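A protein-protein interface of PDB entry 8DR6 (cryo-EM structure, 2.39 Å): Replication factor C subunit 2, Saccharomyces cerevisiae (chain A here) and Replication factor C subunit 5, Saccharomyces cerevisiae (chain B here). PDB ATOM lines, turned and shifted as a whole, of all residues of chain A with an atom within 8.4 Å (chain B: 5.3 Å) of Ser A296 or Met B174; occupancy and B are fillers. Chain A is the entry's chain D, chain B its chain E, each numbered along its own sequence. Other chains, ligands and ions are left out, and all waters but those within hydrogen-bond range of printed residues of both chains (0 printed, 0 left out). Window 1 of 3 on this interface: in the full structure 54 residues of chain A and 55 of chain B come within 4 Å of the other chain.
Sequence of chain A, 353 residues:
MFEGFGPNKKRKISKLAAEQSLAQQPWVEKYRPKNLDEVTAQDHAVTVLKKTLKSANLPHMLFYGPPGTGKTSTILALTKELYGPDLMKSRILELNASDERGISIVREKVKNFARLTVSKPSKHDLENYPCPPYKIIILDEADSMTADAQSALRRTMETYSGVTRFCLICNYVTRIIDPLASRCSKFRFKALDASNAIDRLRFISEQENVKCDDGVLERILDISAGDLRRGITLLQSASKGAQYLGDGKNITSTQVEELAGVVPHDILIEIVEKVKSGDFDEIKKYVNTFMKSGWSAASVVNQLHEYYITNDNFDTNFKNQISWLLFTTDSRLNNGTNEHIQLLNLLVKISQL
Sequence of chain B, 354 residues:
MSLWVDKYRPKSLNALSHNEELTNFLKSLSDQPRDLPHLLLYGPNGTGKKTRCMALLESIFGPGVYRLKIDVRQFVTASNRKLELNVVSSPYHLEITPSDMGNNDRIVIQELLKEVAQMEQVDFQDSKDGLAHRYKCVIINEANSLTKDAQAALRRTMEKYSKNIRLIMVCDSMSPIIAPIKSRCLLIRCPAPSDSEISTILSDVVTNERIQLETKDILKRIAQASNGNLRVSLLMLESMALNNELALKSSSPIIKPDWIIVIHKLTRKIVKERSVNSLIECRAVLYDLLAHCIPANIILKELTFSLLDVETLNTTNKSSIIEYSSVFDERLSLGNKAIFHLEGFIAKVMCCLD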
ATOM      1  N   ALA A 260     -25.106 -16.743 -12.730  1.00  0.00           N
ATOM      2  CA  ALA A 260     -24.173 -15.994 -13.561  1.00  0.00           C
ATOM      3  C   ALA A 260     -23.173 -16.881 -14.289  1.00  0.00           C
ATOM      4  O   ALA A 260     -22.371 -16.366 -15.077  1.00  0.00           O
ATOM      5  CB  ALA A 260     -23.412 -14.974 -12.710  1.00  0.00           C
ATOM      6  N   GLY A 261     -23.196 -18.189 -14.050  1.00  0.00           N
ATOM      7  CA  GLY A 261     -22.276 -19.092 -14.710  1.00  0.00           C
ATOM      8  C   GLY A 261     -20.893 -19.155 -14.104  1.00  0.00           C
ATOM      9  O   GLY A 261     -19.974 -19.670 -14.752  1.00  0.00           O
ATOM     10  N   VAL A 262     -20.711 -18.652 -12.888  1.00  0.00           N
ATOM     11  CA  VAL A 262     -19.408 -18.687 -12.232  1.00  0.00           C
ATOM     12  C   VAL A 262     -19.100 -20.120 -11.820  1.00  0.00           C
ATOM     13  O   VAL A 262     -19.937 -20.799 -11.212  1.00  0.00           O
ATOM     14  CB  VAL A 262     -19.384 -17.742 -11.019  1.00  0.00           C
ATOM     15  CG1 VAL A 262     -18.013 -17.758 -10.360  1.00  0.00           C
ATOM     16  CG2 VAL A 262     -19.763 -16.330 -11.439  1.00  0.00           C
ATOM     17  N   VAL A 263     -17.903 -20.582 -12.152  1.00  0.00           N
ATOM     18  CA  VAL A 263     -17.507 -21.954 -11.817  1.00  0.00           C
ATOM     19  C   VAL A 263     -17.407 -22.090 -10.300  1.00  0.00           C
ATOM     20  O   VAL A 263     -16.881 -21.179  -9.635  1.00  0.00           O
ATOM     21  CB  VAL A 263     -16.178 -22.303 -12.487  1.00  0.00           C
ATOM     22  CG1 VAL A 263     -15.724 -23.699 -12.083  1.00  0.00           C
ATOM     23  CG2 VAL A 263     -16.302 -22.194 -13.998  1.00  0.00           C
ATOM     24  N   PHE A 290     -14.506 -31.477 -18.149  1.00  0.00           N
ATOM     25  CA  PHE A 290     -14.963 -30.164 -17.707  1.00  0.00           C
ATOM     26  C   PHE A 290     -15.787 -29.465 -18.781  1.00  0.00           C
ATOM     27  O   PHE A 290     -16.824 -28.862 -18.480  1.00  0.00           O
ATOM     28  CB  PHE A 290     -13.754 -29.314 -17.311  1.00  0.00           C
ATOM     29  CG  PHE A 290     -14.087 -27.889 -16.972  1.00  0.00           C
ATOM     30  CD1 PHE A 290     -14.060 -26.904 -17.946  1.00  0.00           C
ATOM     31  CD2 PHE A 290     -14.413 -27.531 -15.674  1.00  0.00           C
ATOM     32  CE1 PHE A 290     -14.360 -25.593 -17.633  1.00  0.00           C
ATOM     33  CE2 PHE A 290     -14.714 -26.222 -15.356  1.00  0.00           C
ATOM     34  CZ  PHE A 290     -14.687 -25.251 -16.336  1.00  0.00           C
ATOM     35  N   MET A 291     -15.347 -29.531 -20.040  1.00  0.00           N
ATOM     36  CA  MET A 291     -16.081 -28.858 -21.109  1.00  0.00           C
ATOM     37  C   MET A 291     -17.485 -29.416 -21.297  1.00  0.00           C
ATOM     38  O   MET A 291     -18.323 -28.749 -21.914  1.00  0.00           O
ATOM     39  CB  MET A 291     -15.319 -28.945 -22.434  1.00  0.00           C
ATOM     40  CG  MET A 291     -13.893 -28.422 -22.387  1.00  0.00           C
ATOM     41  SD  MET A 291     -13.794 -26.711 -21.829  1.00  0.00           S
ATOM     42  CE  MET A 291     -14.533 -25.858 -23.220  1.00  0.00           C
ATOM     43  N   SER A 293     -19.708 -29.596 -19.126  1.00  0.00           N
ATOM     44  CA  SER A 293     -20.626 -28.838 -18.288  1.00  0.00           C
ATOM     45  C   SER A 293     -21.041 -27.507 -18.903  1.00  0.00           C
ATOM     46  O   SER A 293     -21.937 -26.847 -18.364  1.00  0.00           O
ATOM     47  CB  SER A 293     -19.995 -28.586 -16.915  1.00  0.00           C
ATOM     48  OG  SER A 293     -19.811 -29.799 -16.209  1.00  0.00           O
ATOM     49  N   GLY A 294     -20.420 -27.096 -20.007  1.00  0.00           N
ATOM     50  CA  GLY A 294     -20.813 -25.881 -20.690  1.00  0.00           C
ATOM     51  C   GLY A 294     -20.259 -24.599 -20.110  1.00  0.00           C
ATOM     52  O   GLY A 294     -20.713 -23.518 -20.502  1.00  0.00           O
ATOM     53  N   TRP A 295     -19.299 -24.676 -19.189  1.00  0.00           N
ATOM     54  CA  TRP A 295     -18.710 -23.469 -18.622  1.00  0.00           C
ATOM     55  C   TRP A 295     -18.072 -22.619 -19.715  1.00  0.00           C
ATOM     56  O   TRP A 295     -17.393 -23.132 -20.608  1.00  0.00           O
ATOM     57  CB  TRP A 295     -17.665 -23.834 -17.566  1.00  0.00           C
ATOM     58  CG  TRP A 295     -18.212 -24.620 -16.416  1.00  0.00           C
ATOM     59  CD1 TRP A 295     -17.925 -25.914 -16.098  1.00  0.00           C
ATOM     60  CD2 TRP A 295     -19.137 -24.159 -15.425  1.00  0.00           C
ATOM     61  NE1 TRP A 295     -18.617 -26.290 -14.972  1.00  0.00           N
ATOM     62  CE2 TRP A 295     -19.367 -25.230 -14.539  1.00  0.00           C
ATOM     63  CE3 TRP A 295     -19.793 -22.945 -15.200  1.00  0.00           C
ATOM     64  CZ2 TRP A 295     -20.226 -25.123 -13.447  1.00  0.00           C
ATOM     65  CZ3 TRP A 295     -20.645 -22.842 -14.116  1.00  0.00           C
ATOM     66  CH2 TRP A 295     -20.854 -23.925 -13.253  1.00  0.00           C
ATOM     67  N   SER A 296     -18.297 -21.310 -19.635  1.00  0.00           N
ATOM     68  CA  SER A 296     -17.715 -20.377 -20.590  1.00  0.00           C
ATOM     69  C   SER A 296     -16.221 -20.229 -20.329  1.00  0.00           C
ATOM     70  O   SER A 296     -15.796 -20.063 -19.182  1.00  0.00           O
ATOM     71  CB  SER A 296     -18.408 -19.019 -20.496  1.00  0.00           C
ATOM     72  OG  SER A 296     -17.815 -18.082 -21.379  1.00  0.00           O
ATOM     73  N   ALA A 297     -15.426 -20.284 -21.399  1.00  0.00           N
ATOM     74  CA  ALA A 297     -13.976 -20.222 -21.247  1.00  0.00           C
ATOM     75  C   ALA A 297     -13.533 -18.889 -20.658  1.00  0.00           C
ATOM     76  O   ALA A 297     -12.579 -18.836 -19.874  1.00  0.00           O
ATOM     77  CB  ALA A 297     -13.297 -20.460 -22.595  1.00  0.00           C
ATOM     78  N   ALA A 298     -14.202 -17.797 -21.035  1.00  0.00           N
ATOM     79  CA  ALA A 298     -13.802 -16.483 -20.543  1.00  0.00           C
ATOM     80  C   ALA A 298     -13.910 -16.406 -19.025  1.00  0.00           C
ATOM     81  O   ALA A 298     -13.018 -15.869 -18.357  1.00  0.00           O
ATOM     82  CB  ALA A 298     -14.656 -15.398 -21.197  1.00  0.00           C
ATOM     83  N   SER A 299     -14.999 -16.934 -18.461  1.00  0.00           N
ATOM     84  CA  SER A 299     -15.157 -16.924 -17.010  1.00  0.00           C
ATOM     85  C   SER A 299     -14.073 -17.754 -16.335  1.00  0.00           C
ATOM     86  O   SER A 299     -13.534 -17.359 -15.294  1.00  0.00           O
ATOM     87  CB  SER A 299     -16.543 -17.443 -16.631  1.00  0.00           C
ATOM     88  OG  SER A 299     -17.512 -17.050 -17.587  1.00  0.00           O
ATOM     89  N   VAL A 300     -13.743 -18.913 -16.909  1.00  0.00           N
ATOM     90  CA  VAL A 300     -12.700 -19.756 -16.336  1.00  0.00           C
ATOM     91  C   VAL A 300     -11.362 -19.028 -16.351  1.00  0.00           C
ATOM     92  O   VAL A 300     -10.605 -19.065 -15.374  1.00  0.00           O
ATOM     93  CB  VAL A 300     -12.618 -21.097 -17.088  1.00  0.00           C
ATOM     94  CG1 VAL A 300     -11.526 -21.975 -16.494  1.00  0.00           C
ATOM     95  CG2 VAL A 300     -13.956 -21.815 -17.047  1.00  0.00           C
ATOM     96  N   VAL A 301     -11.048 -18.359 -17.462  1.00  0.00           N
ATOM     97  CA  VAL A 301      -9.790 -17.627 -17.555  1.00  0.00           C
ATOM     98  C   VAL A 301      -9.756 -16.489 -16.543  1.00  0.00           C
ATOM     99  O   VAL A 301      -8.732 -16.250 -15.893  1.00  0.00           O
ATOM    100  CB  VAL A 301      -9.575 -17.115 -18.991  1.00  0.00           C
ATOM    101  CG1 VAL A 301      -8.373 -16.186 -19.052  1.00  0.00           C
ATOM    102  CG2 VAL A 301      -9.394 -18.283 -19.949  1.00  0.00           C
ATOM    103  N   ASN A 302     -10.868 -15.763 -16.400  1.00  0.00           N
ATOM    104  CA  ASN A 302     -10.911 -14.669 -15.436  1.00  0.00           C
ATOM    105  C   ASN A 302     -10.716 -15.180 -14.013  1.00  0.00           C
ATOM    106  O   ASN A 302      -9.975 -14.581 -13.224  1.00  0.00           O
ATOM    107  CB  ASN A 302     -12.238 -13.918 -15.560  1.00  0.00           C
ATOM    108  CG  ASN A 302     -12.325 -12.729 -14.623  1.00  0.00           C
ATOM    109  OD1 ASN A 302     -11.386 -11.943 -14.510  1.00  0.00           O
ATOM    110  ND2 ASN A 302     -13.459 -12.593 -13.945  1.00  0.00           N
ATOM    111  N   GLN A 303     -11.371 -16.290 -13.668  1.00  0.00           N
ATOM    112  CA  GLN A 303     -11.212 -16.853 -12.331  1.00  0.00           C
ATOM    113  C   GLN A 303      -9.793 -17.359 -12.100  1.00  0.00           C
ATOM    114  O   GLN A 303      -9.250 -17.193 -11.002  1.00  0.00           O
ATOM    115  CB  GLN A 303     -12.222 -17.978 -12.111  1.00  0.00           C
ATOM    116  CG  GLN A 303     -13.647 -17.486 -11.904  1.00  0.00           C
ATOM    117  CD  GLN A 303     -14.639 -18.618 -11.730  1.00  0.00           C
ATOM    118  OE1 GLN A 303     -15.447 -18.893 -12.617  1.00  0.00           O
ATOM    119  NE2 GLN A 303     -14.585 -19.281 -10.581  1.00  0.00           N
ATOM    120  N   LEU A 333      -9.234 -15.874 -27.484  1.00  0.00           N
ATOM    121  CA  LEU A 333     -10.650 -16.164 -27.281  1.00  0.00           C
ATOM    122  C   LEU A 333     -11.533 -15.032 -27.786  1.00  0.00           C
ATOM    123  O   LEU A 333     -12.654 -15.279 -28.243  1.00  0.00           O
ATOM    124  CB  LEU A 333     -10.926 -16.426 -25.801  1.00  0.00           C
ATOM    125  CG  LEU A 333     -10.515 -17.800 -25.267  1.00  0.00           C
ATOM    126  CD1 LEU A 333     -10.569 -17.818 -23.747  1.00  0.00           C
ATOM    127  CD2 LEU A 333     -11.399 -18.894 -25.847  1.00  0.00           C
ATOM    128  N   ASN A 334     -11.052 -13.790 -27.709  1.00  0.00           N
ATOM    129  CA  ASN A 334     -11.833 -12.649 -28.169  1.00  0.00           C
ATOM    130  C   ASN A 334     -12.076 -12.665 -29.672  1.00  0.00           C
ATOM    131  O   ASN A 334     -12.931 -11.912 -30.150  1.00  0.00           O
ATOM    132  CB  ASN A 334     -11.134 -11.346 -27.779  1.00  0.00           C
ATOM    133  CG  ASN A 334     -12.111 -10.257 -27.382  1.00  0.00           C
ATOM    134  OD1 ASN A 334     -12.294  -9.277 -28.105  1.00  0.00           O
ATOM    135  ND2 ASN A 334     -12.743 -10.421 -26.227  1.00  0.00           N
ATOM    136  N   GLY A 336     -13.173 -15.296 -31.345  1.00  0.00           N
ATOM    137  CA  GLY A 336     -14.151 -16.313 -31.673  1.00  0.00           C
ATOM    138  C   GLY A 336     -13.519 -17.640 -32.038  1.00  0.00           C
ATOM    139  O   GLY A 336     -13.758 -18.171 -33.126  1.00  0.00           O
ATOM    140  N   THR A 337     -12.711 -18.184 -31.134  1.00  0.00           N
ATOM    141  CA  THR A 337     -12.002 -19.435 -31.359  1.00  0.00           C
ATOM    142  C   THR A 337     -12.615 -20.554 -30.522  1.00  0.00           C
ATOM    143  O   THR A 337     -13.391 -20.322 -29.592  1.00  0.00           O
ATOM    144  CB  THR A 337     -10.517 -19.276 -31.022  1.00  0.00           C
ATOM    145  OG1 THR A 337     -10.371 -18.493 -29.831  1.00  0.00           O
ATOM    146  CG2 THR A 337      -9.783 -18.596 -32.164  1.00  0.00           C
ATOM    147  N   GLU A 339     -13.174 -23.024 -27.736  1.00  0.00           N
ATOM    148  CA  GLU A 339     -12.837 -22.854 -26.327  1.00  0.00           C
ATOM    149  C   GLU A 339     -12.041 -24.033 -25.784  1.00  0.00           C
ATOM    150  O   GLU A 339     -11.134 -23.842 -24.967  1.00  0.00           O
ATOM    151  CB  GLU A 339     -14.113 -22.655 -25.511  1.00  0.00           C
ATOM    152  CG  GLU A 339     -14.717 -21.268 -25.646  1.00  0.00           C
ATOM    153  CD  GLU A 339     -16.097 -21.168 -25.028  1.00  0.00           C
ATOM    154  OE1 GLU A 339     -16.395 -21.956 -24.106  1.00  0.00           O
ATOM    155  OE2 GLU A 339     -16.884 -20.301 -25.464  1.00  0.00           O
ATOM    156  N   LEU A 343      -8.425 -23.476 -23.988  1.00  0.00           N
ATOM    157  CA  LEU A 343      -8.325 -23.765 -22.562  1.00  0.00           C
ATOM    158  C   LEU A 343      -7.285 -24.845 -22.292  1.00  0.00           C
ATOM    159  O   LEU A 343      -6.488 -24.728 -21.352  1.00  0.00           O
ATOM    160  CB  LEU A 343      -9.690 -24.184 -22.016  1.00  0.00           C
ATOM    161  CG  LEU A 343      -9.742 -24.534 -20.526  1.00  0.00           C
ATOM    162  CD1 LEU A 343      -9.351 -23.336 -19.674  1.00  0.00           C
ATOM    163  CD2 LEU A 343     -11.126 -25.035 -20.144  1.00  0.00           C
ATOM    164  N   LEU B  40     -30.343 -16.370 -24.166  1.00  0.00           N
ATOM    165  CA  LEU B  40     -29.245 -16.944 -24.936  1.00  0.00           C
ATOM    166  C   LEU B  40     -28.858 -18.260 -24.275  1.00  0.00           C
ATOM    167  O   LEU B  40     -28.243 -18.265 -23.204  1.00  0.00           O
ATOM    168  CB  LEU B  40     -28.055 -15.987 -25.000  1.00  0.00           C
ATOM    169  CG  LEU B  40     -26.773 -16.523 -25.644  1.00  0.00           C
ATOM    170  CD1 LEU B  40     -27.075 -17.374 -26.869  1.00  0.00           C
ATOM    171  CD2 LEU B  40     -25.843 -15.376 -26.008  1.00  0.00           C
ATOM    172  N   TYR B  42     -26.665 -21.479 -24.129  1.00  0.00           N
ATOM    173  CA  TYR B  42     -25.367 -21.965 -24.569  1.00  0.00           C
ATOM    174  C   TYR B  42     -25.016 -23.252 -23.835  1.00  0.00           C
ATOM    175  O   TYR B  42     -25.294 -23.403 -22.642  1.00  0.00           O
ATOM    176  CB  TYR B  42     -24.267 -20.918 -24.343  1.00  0.00           C
ATOM    177  CG  TYR B  42     -23.970 -20.633 -22.888  1.00  0.00           C
ATOM    178  CD1 TYR B  42     -24.748 -19.741 -22.162  1.00  0.00           C
ATOM    179  CD2 TYR B  42     -22.909 -21.253 -22.242  1.00  0.00           C
ATOM    180  CE1 TYR B  42     -24.479 -19.477 -20.833  1.00  0.00           C
ATOM    181  CE2 TYR B  42     -22.633 -20.995 -20.913  1.00  0.00           C
ATOM    182  CZ  TYR B  42     -23.421 -20.106 -20.214  1.00  0.00           C
ATOM    183  OH  TYR B  42     -23.149 -19.846 -18.890  1.00  0.00           O
ATOM    184  N   CYS B 171     -26.899 -21.288 -29.045  1.00  0.00           N
ATOM    185  CA  CYS B 171     -25.533 -21.382 -29.538  1.00  0.00           C
ATOM    186  C   CYS B 171     -24.803 -22.488 -28.791  1.00  0.00           C
ATOM    187  O   CYS B 171     -25.201 -22.897 -27.699  1.00  0.00           O
ATOM    188  CB  CYS B 171     -24.783 -20.052 -29.378  1.00  0.00           C
ATOM    189  SG  CYS B 171     -24.355 -19.642 -27.670  1.00  0.00           S
ATOM    190  N   ASP B 172     -23.725 -22.977 -29.405  1.00  0.00           N
ATOM    191  CA  ASP B 172     -22.860 -23.961 -28.766  1.00  0.00           C
ATOM    192  C   ASP B 172     -21.680 -23.329 -28.043  1.00  0.00           C
ATOM    193  O   ASP B 172     -21.153 -23.935 -27.103  1.00  0.00           O
ATOM    194  CB  ASP B 172     -22.332 -24.963 -29.802  1.00  0.00           C
ATOM    195  CG  ASP B 172     -21.733 -24.289 -31.021  1.00  0.00           C
ATOM    196  OD1 ASP B 172     -22.032 -24.728 -32.151  1.00  0.00           O
ATOM    197  OD2 ASP B 172     -20.964 -23.320 -30.850  1.00  0.00           O
ATOM    198  N   SER B 173     -21.259 -22.135 -28.455  1.00  0.00           N
ATOM    199  CA  SER B 173     -20.184 -21.417 -27.789  1.00  0.00           C
ATOM    200  C   SER B 173     -20.463 -19.925 -27.887  1.00  0.00           C
ATOM    201  O   SER B 173     -20.933 -19.434 -28.917  1.00  0.00           O
ATOM    202  CB  SER B 173     -18.818 -21.745 -28.403  1.00  0.00           C
ATOM    203  OG  SER B 173     -17.820 -20.859 -27.927  1.00  0.00           O
ATOM    204  N   MET B 174     -20.170 -19.209 -26.804  1.00  0.00           N
ATOM    205  CA  MET B 174     -20.412 -17.776 -26.726  1.00  0.00           C
ATOM    206  C   MET B 174     -19.209 -16.946 -27.154  1.00  0.00           C
ATOM    207  O   MET B 174     -19.298 -15.714 -27.163  1.00  0.00           O
ATOM    208  CB  MET B 174     -20.818 -17.391 -25.299  1.00  0.00           C
ATOM    209  CG  MET B 174     -22.263 -17.724 -24.960  1.00  0.00           C
ATOM    210  SD  MET B 174     -22.809 -17.115 -23.349  1.00  0.00           S
ATOM    211  CE  MET B 174     -21.311 -17.241 -22.373  1.00  0.00           C
ATOM    212  N   SER B 175     -18.094 -17.584 -27.504  1.00  0.00           N
ATOM    213  CA  SER B 175     -16.919 -16.824 -27.917  1.00  0.00           C
ATOM    214  C   SER B 175     -17.172 -15.964 -29.150  1.00  0.00           C
ATOM    215  O   SER B 175     -16.745 -14.796 -29.149  1.00  0.00           O
ATOM    216  CB  SER B 175     -15.741 -17.780 -28.152  1.00  0.00           C
ATOM    217  OG  SER B 175     -15.651 -18.176 -29.509  1.00  0.00           O
ATOM    218  N   PRO B 176     -17.835 -16.446 -30.207  1.00  0.00           N
ATOM    219  CA  PRO B 176     -18.043 -15.598 -31.390  1.00  0.00           C
ATOM    220  C   PRO B 176     -19.069 -14.493 -31.196  1.00  0.00           C
ATOM    221  O   PRO B 176     -19.150 -13.597 -32.046  1.00  0.00           O
ATOM    222  CB  PRO B 176     -18.516 -16.600 -32.462  1.00  0.00           C
ATOM    223  CG  PRO B 176     -18.278 -17.970 -31.874  1.00  0.00           C
ATOM    224  CD  PRO B 176     -18.411 -17.784 -30.405  1.00  0.00           C
ATOM    225  N   ILE B 177     -19.849 -14.523 -30.119  1.00  0.00           N
ATOM    226  CA  ILE B 177     -20.878 -13.521 -29.873  1.00  0.00           C
ATOM    227  C   ILE B 177     -20.220 -12.265 -29.319  1.00  0.00           C
ATOM    228  O   ILE B 177     -19.436 -12.331 -28.365  1.00  0.00           O
ATOM    229  CB  ILE B 177     -21.948 -14.055 -28.904  1.00  0.00           C
ATOM    230  CG1 ILE B 177     -22.485 -15.408 -29.380  1.00  0.00           C
ATOM    231  CG2 ILE B 177     -23.082 -13.048 -28.763  1.00  0.00           C
ATOM    232  CD1 ILE B 177     -23.195 -15.362 -30.721  1.00  0.00           C
ATOM    233  N   LYS B 182     -24.265 -10.131 -25.923  1.00  0.00           N
ATOM    234  CA  LYS B 182     -24.303 -10.908 -24.689  1.00  0.00           C
ATOM    235  C   LYS B 182     -24.812 -10.073 -23.524  1.00  0.00           C
ATOM    236  O   LYS B 182     -25.423 -10.611 -22.593  1.00  0.00           O
ATOM    237  CB  LYS B 182     -22.913 -11.463 -24.377  1.00  0.00           C
ATOM    238  CG  LYS B 182     -22.564 -12.725 -25.149  1.00  0.00           C
ATOM    239  CD  LYS B 182     -21.060 -12.873 -25.345  1.00  0.00           C
ATOM    240  CE  LYS B 182     -20.307 -12.828 -24.023  1.00  0.00           C
ATOM    241  NZ  LYS B 182     -20.804 -13.847 -23.061  1.00  0.00           N
ATOM    242  N   LEU B 187     -28.164 -15.194 -20.054  1.00  0.00           N
ATOM    243  CA  LEU B 187     -27.367 -16.343 -20.464  1.00  0.00           C
ATOM    244  C   LEU B 187     -27.778 -17.564 -19.648  1.00  0.00           C
ATOM    245  O   LEU B 187     -27.773 -17.522 -18.413  1.00  0.00           O
ATOM    246  CB  LEU B 187     -25.879 -16.048 -20.286  1.00  0.00           C
ATOM    247  CG  LEU B 187     -25.402 -14.715 -20.868  1.00  0.00           C
ATOM    248  CD1 LEU B 187     -23.888 -14.599 -20.773  1.00  0.00           C
ATOM    249  CD2 LEU B 187     -25.863 -14.554 -22.310  1.00  0.00           C
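The side-chain hydroxyl of Ser B173 is in hydrogen-bond range of the side-chain carboxylate of Glu A339 (2.7 Å). OG of Ser B175 sits at hydrogen-bond distance from O of Thr A337.
N of Ser B175 sits at hydrogen-bond distance from OG of Ser B173 (3.3 Å). OE1 of Glu A339 sits at hydrogen-bond distance from N of Ala A297, 3.3 Å away. SG of Cys B171 lies within hydrogen-bond range of O of Ser B173, 3.6 Å away.
Gly A294 touches Tyr B42 (O to CE2, 3.2 Å). Met B174 touches Ser A296. O of Leu A333 touches CB of Ser B175, at 3.97 Å. Ser B175 touches Gly A336. N of Pro B176 touches CA of Gly A336 (3.97 Å). Glu A339 touches Met B174 (OE2 to N, 3.7 Å). OE2 of Glu A339 touches N of Ser B175, at 3.6 Å.
Printed residues of chain B within 4 Å of Gly A294: Tyr B42. Ser A296 touches one residue of chain B. Printed residues of chain B within 4 Å of Gly A336: Ser B175 (3.2 Å) and Pro B176 (3.97 Å). Of the printed residues of chain B, Thr A337 touches Ser B175 (3.1 Å). Of the printed residues of chain A, Tyr B42 touches Gly A294 (3.2 Å). Ser B173 touches just one residue of chain A: Glu A339. Of the printed residues of chain A, Met B174 touches Ser A296 (3.7 Å) and Glu A339 (3.7 Å). Printed residues of chain A within 4 Å of Pro B176: Gly A336 (3.97 Å). The nearest residue of chain B that does not touch Ser A296 is Tyr B42 (4.5 Å).
Printed residues of chain A that touch a printed residue of chain B: Gly A294, Ser A296, Leu A333, Gly A336, Thr A337 and Glu A339. Of the 11 printed residues of chain B, 5 touch a printed residue of chain A. Printed residues of chain B that touch a printed residue of chain A: Tyr B42, Ser B173, Met B174, Ser B175 and Pro B176. Hydrophobic or aromatic side chains of chain B within 4 Å of the printed part of chain A: Tyr B42 and Met B174. Along chain B the printed residues that touch a printed residue of chain A span positions 42 to 176. Among the printed residues, 9 pairs touch across the chains.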
